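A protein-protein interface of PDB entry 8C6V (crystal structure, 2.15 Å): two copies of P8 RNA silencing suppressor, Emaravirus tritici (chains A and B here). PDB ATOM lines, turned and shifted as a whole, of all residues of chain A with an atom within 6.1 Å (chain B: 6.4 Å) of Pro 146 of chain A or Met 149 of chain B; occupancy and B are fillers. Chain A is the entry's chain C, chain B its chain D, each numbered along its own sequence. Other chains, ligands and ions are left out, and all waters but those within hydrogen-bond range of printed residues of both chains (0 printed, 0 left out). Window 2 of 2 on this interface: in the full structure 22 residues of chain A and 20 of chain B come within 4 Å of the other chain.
Of chain B, only Met 149 (3.8 Å) comes within 4 Å of Pro 146 of chain A.
Printed residues of chain B within 4 Å of Met 149 of chain A: Cys 148 (3.4 Å), Met 149 (3.8 Å) and Asn 152 (3.8 Å).
Printed residues of chain A within 4 Å of Cys 148 of chain B: Met 149.
Of chain A, only Pro 146, Cys 148 and Met 149 come within 4 Å of Met 149 of chain B.
Printed residues of chain A within 4 Å of Asn 152 of chain B: Met 149, Asn 152 and Gln 153.
The nearest residue of chain A that does not touch Met 149 of chain B is Asn 152 of chain A (5.5 Å).
The nearest printed residue of chain B that does not touch Gln 153 of chain A is Cys 148 of chain B (7.8 Å).
Cys 148 of chain A touches Met 149 of chain B, and with the chains exchanged Met 149 of chain A touches Cys 148 of chain B.
Met 149 of chain A touches Asn 152 of chain B, but with the chains exchanged Asn 152 of chain A does not touch Met 149 of chain B (5.5 Å).
Asn 152 of chain B touches its own counterpart, Asn 152 of chain A.
Asn 152 of chain A touches Gln 153 of chain B, and with the chains exchanged Gln 153 of chain A touches Asn 152 of chain B.
9 positions are printed for both chains.
Of the 8 pairs that touch across the chains among the printed residues, 6 have their exchanged pair printed and touching as well.
SG of Cys 148 of chain A sits at hydrogen-bond distance from SD of Met 149 of chain B.
SD of Met 149 of chain A is in hydrogen-bond range of SG of Cys 148 of chain B.
ND2 of Asn 152 of chain A lies within hydrogen-bond range of OD1 of Asn 152 of chain B (2.9 Å).
The side-chain amide nitrogen of Gln 145 of chain B lies within hydrogen-bond range of the side-chain amide oxygen of Gln 153 of chain B, 2.7 Å away.
O of Met 149 of chain B lies close to OE1 of Gln 153 of chain B (3.4 Å).
The backbone carbonyl oxygen of Met 149 of chain A lies close to the side-chain amide oxygen of Gln 153 of chain A, at 3.3 Å.
The side-chain amide nitrogen (NE2) of Gln 145 of chain A is in hydrogen-bond range of the side-chain amide oxygen (OE1) of Gln 153 of chain A (2.5 Å).
CE of Met 149 of chain B touches CG of Pro 146 of chain A (3.8 Å).
CG of Met 149 of chain A touches CG of Met 149 of chain B, at 3.8 Å.
O of Met 149 of chain A touches ND2 of Asn 152 of chain B, 3.8 Å away.
Asn 152 of chain A touches Gln 153 of chain B (ND2 to CG, 3.96 Å).
Asn 152 of chain B touches Gln 153 of chain A (ND2 to CG, 3.8 Å).
Hydrophobic or aromatic side chains of chain B that line the printed part of chain A: Met 149.
Hydrophobic or aromatic side chains of chain A within 4 Å of the printed part of chain B: Pro 146 and Met 149.
Along chain A the printed residues that touch a printed residue of chain B span positions 146 to 153.
Among the printed residues, 8 pairs touch across the chains.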
ATOM      1  N   HIS A 142     -13.382   3.992  -0.209  1.00  0.00           N
ATOM      2  CA  HIS A 142     -13.048   5.028  -1.179  1.00  0.00           C
ATOM      3  C   HIS A 142     -14.283   5.462  -1.958  1.00  0.00           C
ATOM      4  O   HIS A 142     -14.577   6.658  -2.057  1.00  0.00           O
ATOM      5  CB  HIS A 142     -11.953   4.520  -2.122  1.00  0.00           C
ATOM      6  CG  HIS A 142     -11.657   5.434  -3.273  1.00  0.00           C
ATOM      7  ND1 HIS A 142     -11.054   4.994  -4.431  1.00  0.00           N
ATOM      8  CD2 HIS A 142     -11.870   6.761  -3.443  1.00  0.00           C
ATOM      9  CE1 HIS A 142     -10.913   6.006  -5.268  1.00  0.00           C
ATOM     10  NE2 HIS A 142     -11.404   7.090  -4.693  1.00  0.00           N
ATOM     11  N   GLN A 144     -17.402   5.273  -1.339  1.00  0.00           N
ATOM     12  CA  GLN A 144     -18.479   5.837  -0.534  1.00  0.00           C
ATOM     13  C   GLN A 144     -18.104   7.153   0.135  1.00  0.00           C
ATOM     14  O   GLN A 144     -18.988   7.834   0.663  1.00  0.00           O
ATOM     15  CB  GLN A 144     -18.912   4.837   0.548  1.00  0.00           C
ATOM     16  CG  GLN A 144     -19.368   3.490   0.016  1.00  0.00           C
ATOM     17  CD  GLN A 144     -20.637   3.588  -0.802  1.00  0.00           C
ATOM     18  OE1 GLN A 144     -21.629   4.169  -0.363  1.00  0.00           O
ATOM     19  NE2 GLN A 144     -20.611   3.021  -2.002  1.00  0.00           N
ATOM     20  N   GLN A 145     -16.827   7.517   0.134  1.00  0.00           N
ATOM     21  CA  GLN A 145     -16.371   8.696   0.860  1.00  0.00           C
ATOM     22  C   GLN A 145     -16.729   9.967   0.098  1.00  0.00           C
ATOM     23  O   GLN A 145     -16.509  10.037  -1.116  1.00  0.00           O
ATOM     24  CB  GLN A 145     -14.862   8.632   1.083  1.00  0.00           C
ATOM     25  CG  GLN A 145     -14.334   9.563   2.167  1.00  0.00           C
ATOM     26  CD  GLN A 145     -14.467   8.979   3.561  1.00  0.00           C
ATOM     27  OE1 GLN A 145     -15.466   8.336   3.888  1.00  0.00           O
ATOM     28  NE2 GLN A 145     -13.451   9.191   4.389  1.00  0.00           N
ATOM     29  N   PRO A 146     -17.269  10.984   0.766  1.00  0.00           N
ATOM     30  CA  PRO A 146     -17.479  12.270   0.095  1.00  0.00           C
ATOM     31  C   PRO A 146     -16.157  12.975  -0.166  1.00  0.00           C
ATOM     32  O   PRO A 146     -15.186  12.831   0.582  1.00  0.00           O
ATOM     33  CB  PRO A 146     -18.356  13.060   1.077  1.00  0.00           C
ATOM     34  CG  PRO A 146     -18.360  12.293   2.363  1.00  0.00           C
ATOM     35  CD  PRO A 146     -17.573  11.032   2.206  1.00  0.00           C
ATOM     36  N   GLY A 147     -16.136  13.750  -1.254  1.00  0.00           N
ATOM     37  CA  GLY A 147     -14.885  14.312  -1.740  1.00  0.00           C
ATOM     38  C   GLY A 147     -14.192  15.230  -0.752  1.00  0.00           C
ATOM     39  O   GLY A 147     -12.960  15.279  -0.708  1.00  0.00           O
ATOM     40  N   CYS A 148     -14.962  15.970   0.048  1.00  0.00           N
ATOM     41  CA  CYS A 148     -14.351  16.885   1.007  1.00  0.00           C
ATOM     42  C   CYS A 148     -13.628  16.138   2.119  1.00  0.00           C
ATOM     43  O   CYS A 148     -12.630  16.638   2.651  1.00  0.00           O
ATOM     44  CB  CYS A 148     -15.410  17.820   1.591  1.00  0.00           C
ATOM     45  SG  CYS A 148     -16.761  16.977   2.434  1.00  0.00           S
ATOM     46  N   MET A 149     -14.113  14.950   2.489  1.00  0.00           N
ATOM     47  CA  MET A 149     -13.376  14.116   3.431  1.00  0.00           C
ATOM     48  C   MET A 149     -12.098  13.586   2.796  1.00  0.00           C
ATOM     49  O   MET A 149     -11.029  13.603   3.418  1.00  0.00           O
ATOM     50  CB  MET A 149     -14.249  12.958   3.915  1.00  0.00           C
ATOM     51  CG  MET A 149     -15.423  13.371   4.780  1.00  0.00           C
ATOM     52  SD  MET A 149     -16.350  11.960   5.418  1.00  0.00           S
ATOM     53  CE  MET A 149     -15.189  11.281   6.601  1.00  0.00           C
ATOM     54  N   LEU A 150     -12.195  13.110   1.551  1.00  0.00           N
ATOM     55  CA  LEU A 150     -11.021  12.590   0.859  1.00  0.00           C
ATOM     56  C   LEU A 150      -9.945  13.658   0.717  1.00  0.00           C
ATOM     57  O   LEU A 150      -8.752  13.370   0.867  1.00  0.00           O
ATOM     58  CB  LEU A 150     -11.419  12.047  -0.513  1.00  0.00           C
ATOM     59  CG  LEU A 150     -12.195  10.730  -0.544  1.00  0.00           C
ATOM     60  CD1 LEU A 150     -12.585  10.374  -1.971  1.00  0.00           C
ATOM     61  CD2 LEU A 150     -11.373   9.613   0.084  1.00  0.00           C
ATOM     62  N   MET A 151     -10.345  14.901   0.440  1.00  0.00           N
ATOM     63  CA  MET A 151      -9.361  15.957   0.234  1.00  0.00           C
ATOM     64  C   MET A 151      -8.628  16.304   1.528  1.00  0.00           C
ATOM     65  O   MET A 151      -7.469  16.729   1.482  1.00  0.00           O
ATOM     66  CB  MET A 151     -10.036  17.194  -0.354  1.00  0.00           C
ATOM     67  CG  MET A 151     -10.389  18.229   0.680  1.00  0.00           C
ATOM     68  SD  MET A 151     -11.733  19.320   0.219  1.00  0.00           S
ATOM     69  CE  MET A 151     -12.190  19.848   1.858  1.00  0.00           C
ATOM     70  N   ASN A 152      -9.280  16.133   2.685  1.00  0.00           N
ATOM     71  CA  ASN A 152      -8.577  16.310   3.952  1.00  0.00           C
ATOM     72  C   ASN A 152      -7.655  15.134   4.240  1.00  0.00           C
ATOM     73  O   ASN A 152      -6.596  15.313   4.852  1.00  0.00           O
ATOM     74  CB  ASN A 152      -9.570  16.491   5.100  1.00  0.00           C
ATOM     75  CG  ASN A 152     -10.119  17.902   5.186  1.00  0.00           C
ATOM     76  OD1 ASN A 152      -9.572  18.833   4.596  1.00  0.00           O
ATOM     77  ND2 ASN A 152     -11.204  18.069   5.935  1.00  0.00           N
ATOM     78  N   GLN A 153      -8.039  13.931   3.810  1.00  0.00           N
ATOM     79  CA  GLN A 153      -7.156  12.779   3.943  1.00  0.00           C
ATOM     80  C   GLN A 153      -5.948  12.899   3.023  1.00  0.00           C
ATOM     81  O   GLN A 153      -4.856  12.435   3.371  1.00  0.00           O
ATOM     82  CB  GLN A 153      -7.938  11.496   3.659  1.00  0.00           C
ATOM     83  CG  GLN A 153      -9.098  11.269   4.617  1.00  0.00           C
ATOM     84  CD  GLN A 153     -10.043  10.175   4.156  1.00  0.00           C
ATOM     85  OE1 GLN A 153     -11.244  10.401   4.005  1.00  0.00           O
ATOM     86  NE2 GLN A 153      -9.507   8.980   3.934  1.00  0.00           N
ATOM     87  N   TYR B 108     -14.715  24.258  14.372  1.00  0.00           N
ATOM     88  CA  TYR B 108     -14.101  23.334  13.433  1.00  0.00           C
ATOM     89  C   TYR B 108     -13.484  24.118  12.285  1.00  0.00           C
ATOM     90  O   TYR B 108     -13.946  25.209  11.938  1.00  0.00           O
ATOM     91  CB  TYR B 108     -15.118  22.334  12.877  1.00  0.00           C
ATOM     92  CG  TYR B 108     -15.690  21.385  13.902  1.00  0.00           C
ATOM     93  CD1 TYR B 108     -16.785  21.744  14.677  1.00  0.00           C
ATOM     94  CD2 TYR B 108     -15.143  20.124  14.082  1.00  0.00           C
ATOM     95  CE1 TYR B 108     -17.314  20.872  15.612  1.00  0.00           C
ATOM     96  CE2 TYR B 108     -15.663  19.247  15.010  1.00  0.00           C
ATOM     97  CZ  TYR B 108     -16.746  19.623  15.772  1.00  0.00           C
ATOM     98  OH  TYR B 108     -17.254  18.739  16.694  1.00  0.00           O
ATOM     99  N   GLN B 145     -23.048  20.646   8.643  1.00  0.00           N
ATOM    100  CA  GLN B 145     -22.027  19.658   8.307  1.00  0.00           C
ATOM    101  C   GLN B 145     -22.396  18.289   8.868  1.00  0.00           C
ATOM    102  O   GLN B 145     -22.729  18.181  10.054  1.00  0.00           O
ATOM    103  CB  GLN B 145     -20.666  20.085   8.842  1.00  0.00           C
ATOM    104  CG  GLN B 145     -19.482  19.351   8.212  1.00  0.00           C
ATOM    105  CD  GLN B 145     -19.125  19.871   6.826  1.00  0.00           C
ATOM    106  OE1 GLN B 145     -20.000  20.209   6.027  1.00  0.00           O
ATOM    107  NE2 GLN B 145     -17.831  19.946   6.540  1.00  0.00           N
ATOM    108  N   PRO B 146     -22.355  17.236   8.052  1.00  0.00           N
ATOM    109  CA  PRO B 146     -22.581  15.885   8.580  1.00  0.00           C
ATOM    110  C   PRO B 146     -21.533  15.510   9.617  1.00  0.00           C
ATOM    111  O   PRO B 146     -20.412  16.022   9.617  1.00  0.00           O
ATOM    112  CB  PRO B 146     -22.479  14.996   7.336  1.00  0.00           C
ATOM    113  CG  PRO B 146     -22.796  15.909   6.194  1.00  0.00           C
ATOM    114  CD  PRO B 146     -22.237  17.245   6.585  1.00  0.00           C
ATOM    115  N   GLY B 147     -21.914  14.585  10.501  1.00  0.00           N
ATOM    116  CA  GLY B 147     -21.056  14.244  11.625  1.00  0.00           C
ATOM    117  C   GLY B 147     -19.746  13.597  11.216  1.00  0.00           C
ATOM    118  O   GLY B 147     -18.707  13.843  11.835  1.00  0.00           O
ATOM    119  N   CYS B 148     -19.774  12.755  10.178  1.00  0.00           N
ATOM    120  CA  CYS B 148     -18.542  12.109   9.731  1.00  0.00           C
ATOM    121  C   CYS B 148     -17.541  13.120   9.188  1.00  0.00           C
ATOM    122  O   CYS B 148     -16.329  12.920   9.318  1.00  0.00           O
ATOM    123  CB  CYS B 148     -18.850  11.054   8.671  1.00  0.00           C
ATOM    124  SG  CYS B 148     -19.433  11.742   7.107  1.00  0.00           S
ATOM    125  N   MET B 149     -18.021  14.204   8.576  1.00  0.00           N
ATOM    126  CA  MET B 149     -17.111  15.229   8.074  1.00  0.00           C
ATOM    127  C   MET B 149     -16.481  16.007   9.223  1.00  0.00           C
ATOM    128  O   MET B 149     -15.269  16.254   9.226  1.00  0.00           O
ATOM    129  CB  MET B 149     -17.851  16.172   7.126  1.00  0.00           C
ATOM    130  CG  MET B 149     -18.366  15.509   5.858  1.00  0.00           C
ATOM    131  SD  MET B 149     -19.253  16.658   4.784  1.00  0.00           S
ATOM    132  CE  MET B 149     -19.879  15.538   3.535  1.00  0.00           C
ATOM    133  N   LEU B 150     -17.292  16.398  10.210  1.00  0.00           N
ATOM    134  CA  LEU B 150     -16.763  17.126  11.360  1.00  0.00           C
ATOM    135  C   LEU B 150     -15.717  16.305  12.103  1.00  0.00           C
ATOM    136  O   LEU B 150     -14.717  16.851  12.582  1.00  0.00           O
ATOM    137  CB  LEU B 150     -17.901  17.521  12.301  1.00  0.00           C
ATOM    138  CG  LEU B 150     -18.851  18.608  11.798  1.00  0.00           C
ATOM    139  CD1 LEU B 150     -19.987  18.815  12.786  1.00  0.00           C
ATOM    140  CD2 LEU B 150     -18.101  19.913  11.555  1.00  0.00           C
ATOM    141  N   MET B 151     -15.916  14.990  12.202  1.00  0.00           N
ATOM    142  CA  MET B 151     -14.922  14.171  12.885  1.00  0.00           C
ATOM    143  C   MET B 151     -13.644  14.041  12.067  1.00  0.00           C
ATOM    144  O   MET B 151     -12.561  13.870  12.636  1.00  0.00           O
ATOM    145  CB  MET B 151     -15.502  12.796  13.211  1.00  0.00           C
ATOM    146  CG  MET B 151     -16.588  12.830  14.277  1.00  0.00           C
ATOM    147  SD  MET B 151     -16.078  13.619  15.822  1.00  0.00           S
ATOM    148  CE  MET B 151     -16.825  15.244  15.662  1.00  0.00           C
ATOM    149  N   ASN B 152     -13.744  14.128  10.739  1.00  0.00           N
ATOM    150  CA  ASN B 152     -12.540  14.163   9.921  1.00  0.00           C
ATOM    151  C   ASN B 152     -11.822  15.503  10.057  1.00  0.00           C
ATOM    152  O   ASN B 152     -10.586  15.556  10.042  1.00  0.00           O
ATOM    153  CB  ASN B 152     -12.893  13.875   8.464  1.00  0.00           C
ATOM    154  CG  ASN B 152     -11.791  14.272   7.511  1.00  0.00           C
ATOM    155  OD1 ASN B 152     -11.719  15.421   7.078  1.00  0.00           O
ATOM    156  ND2 ASN B 152     -10.922  13.325   7.177  1.00  0.00           N
ATOM    157  N   GLN B 153     -12.578  16.596  10.199  1.00  0.00           N
ATOM    158  CA  GLN B 153     -11.960  17.912  10.347  1.00  0.00           C
ATOM    159  C   GLN B 153     -11.211  18.030  11.668  1.00  0.00           C
ATOM    160  O   GLN B 153     -10.120  18.611  11.721  1.00  0.00           O
ATOM    161  CB  GLN B 153     -13.018  19.010  10.235  1.00  0.00           C
ATOM    162  CG  GLN B 153     -13.655  19.118   8.857  1.00  0.00           C
ATOM    163  CD  GLN B 153     -14.901  19.986   8.844  1.00  0.00           C
ATOM    164  OE1 GLN B 153     -15.998  19.513   8.542  1.00  0.00           O
ATOM    165  NE2 GLN B 153     -14.738  21.265   9.164  1.00  0.00           N
ATOM    166  N   ILE B 154     -11.781  17.493  12.749  1.00  0.00           N
ATOM    167  CA  ILE B 154     -11.099  17.567  14.036  1.00  0.00           C
ATOM    168  C   ILE B 154      -9.938  16.578  14.083  1.00  0.00           C
ATOM    169  O   ILE B 154      -8.956  16.798  14.802  1.00  0.00           O
ATOM    170  CB  ILE B 154     -12.101  17.343  15.187  1.00  0.00           C
ATOM    171  CG1 ILE B 154     -11.490  17.759  16.527  1.00  0.00           C
ATOM    172  CG2 ILE B 154     -12.554  15.898  15.244  1.00  0.00           C
ATOM    173  CD1 ILE B 154     -11.295  19.252  16.670  1.00  0.00           C
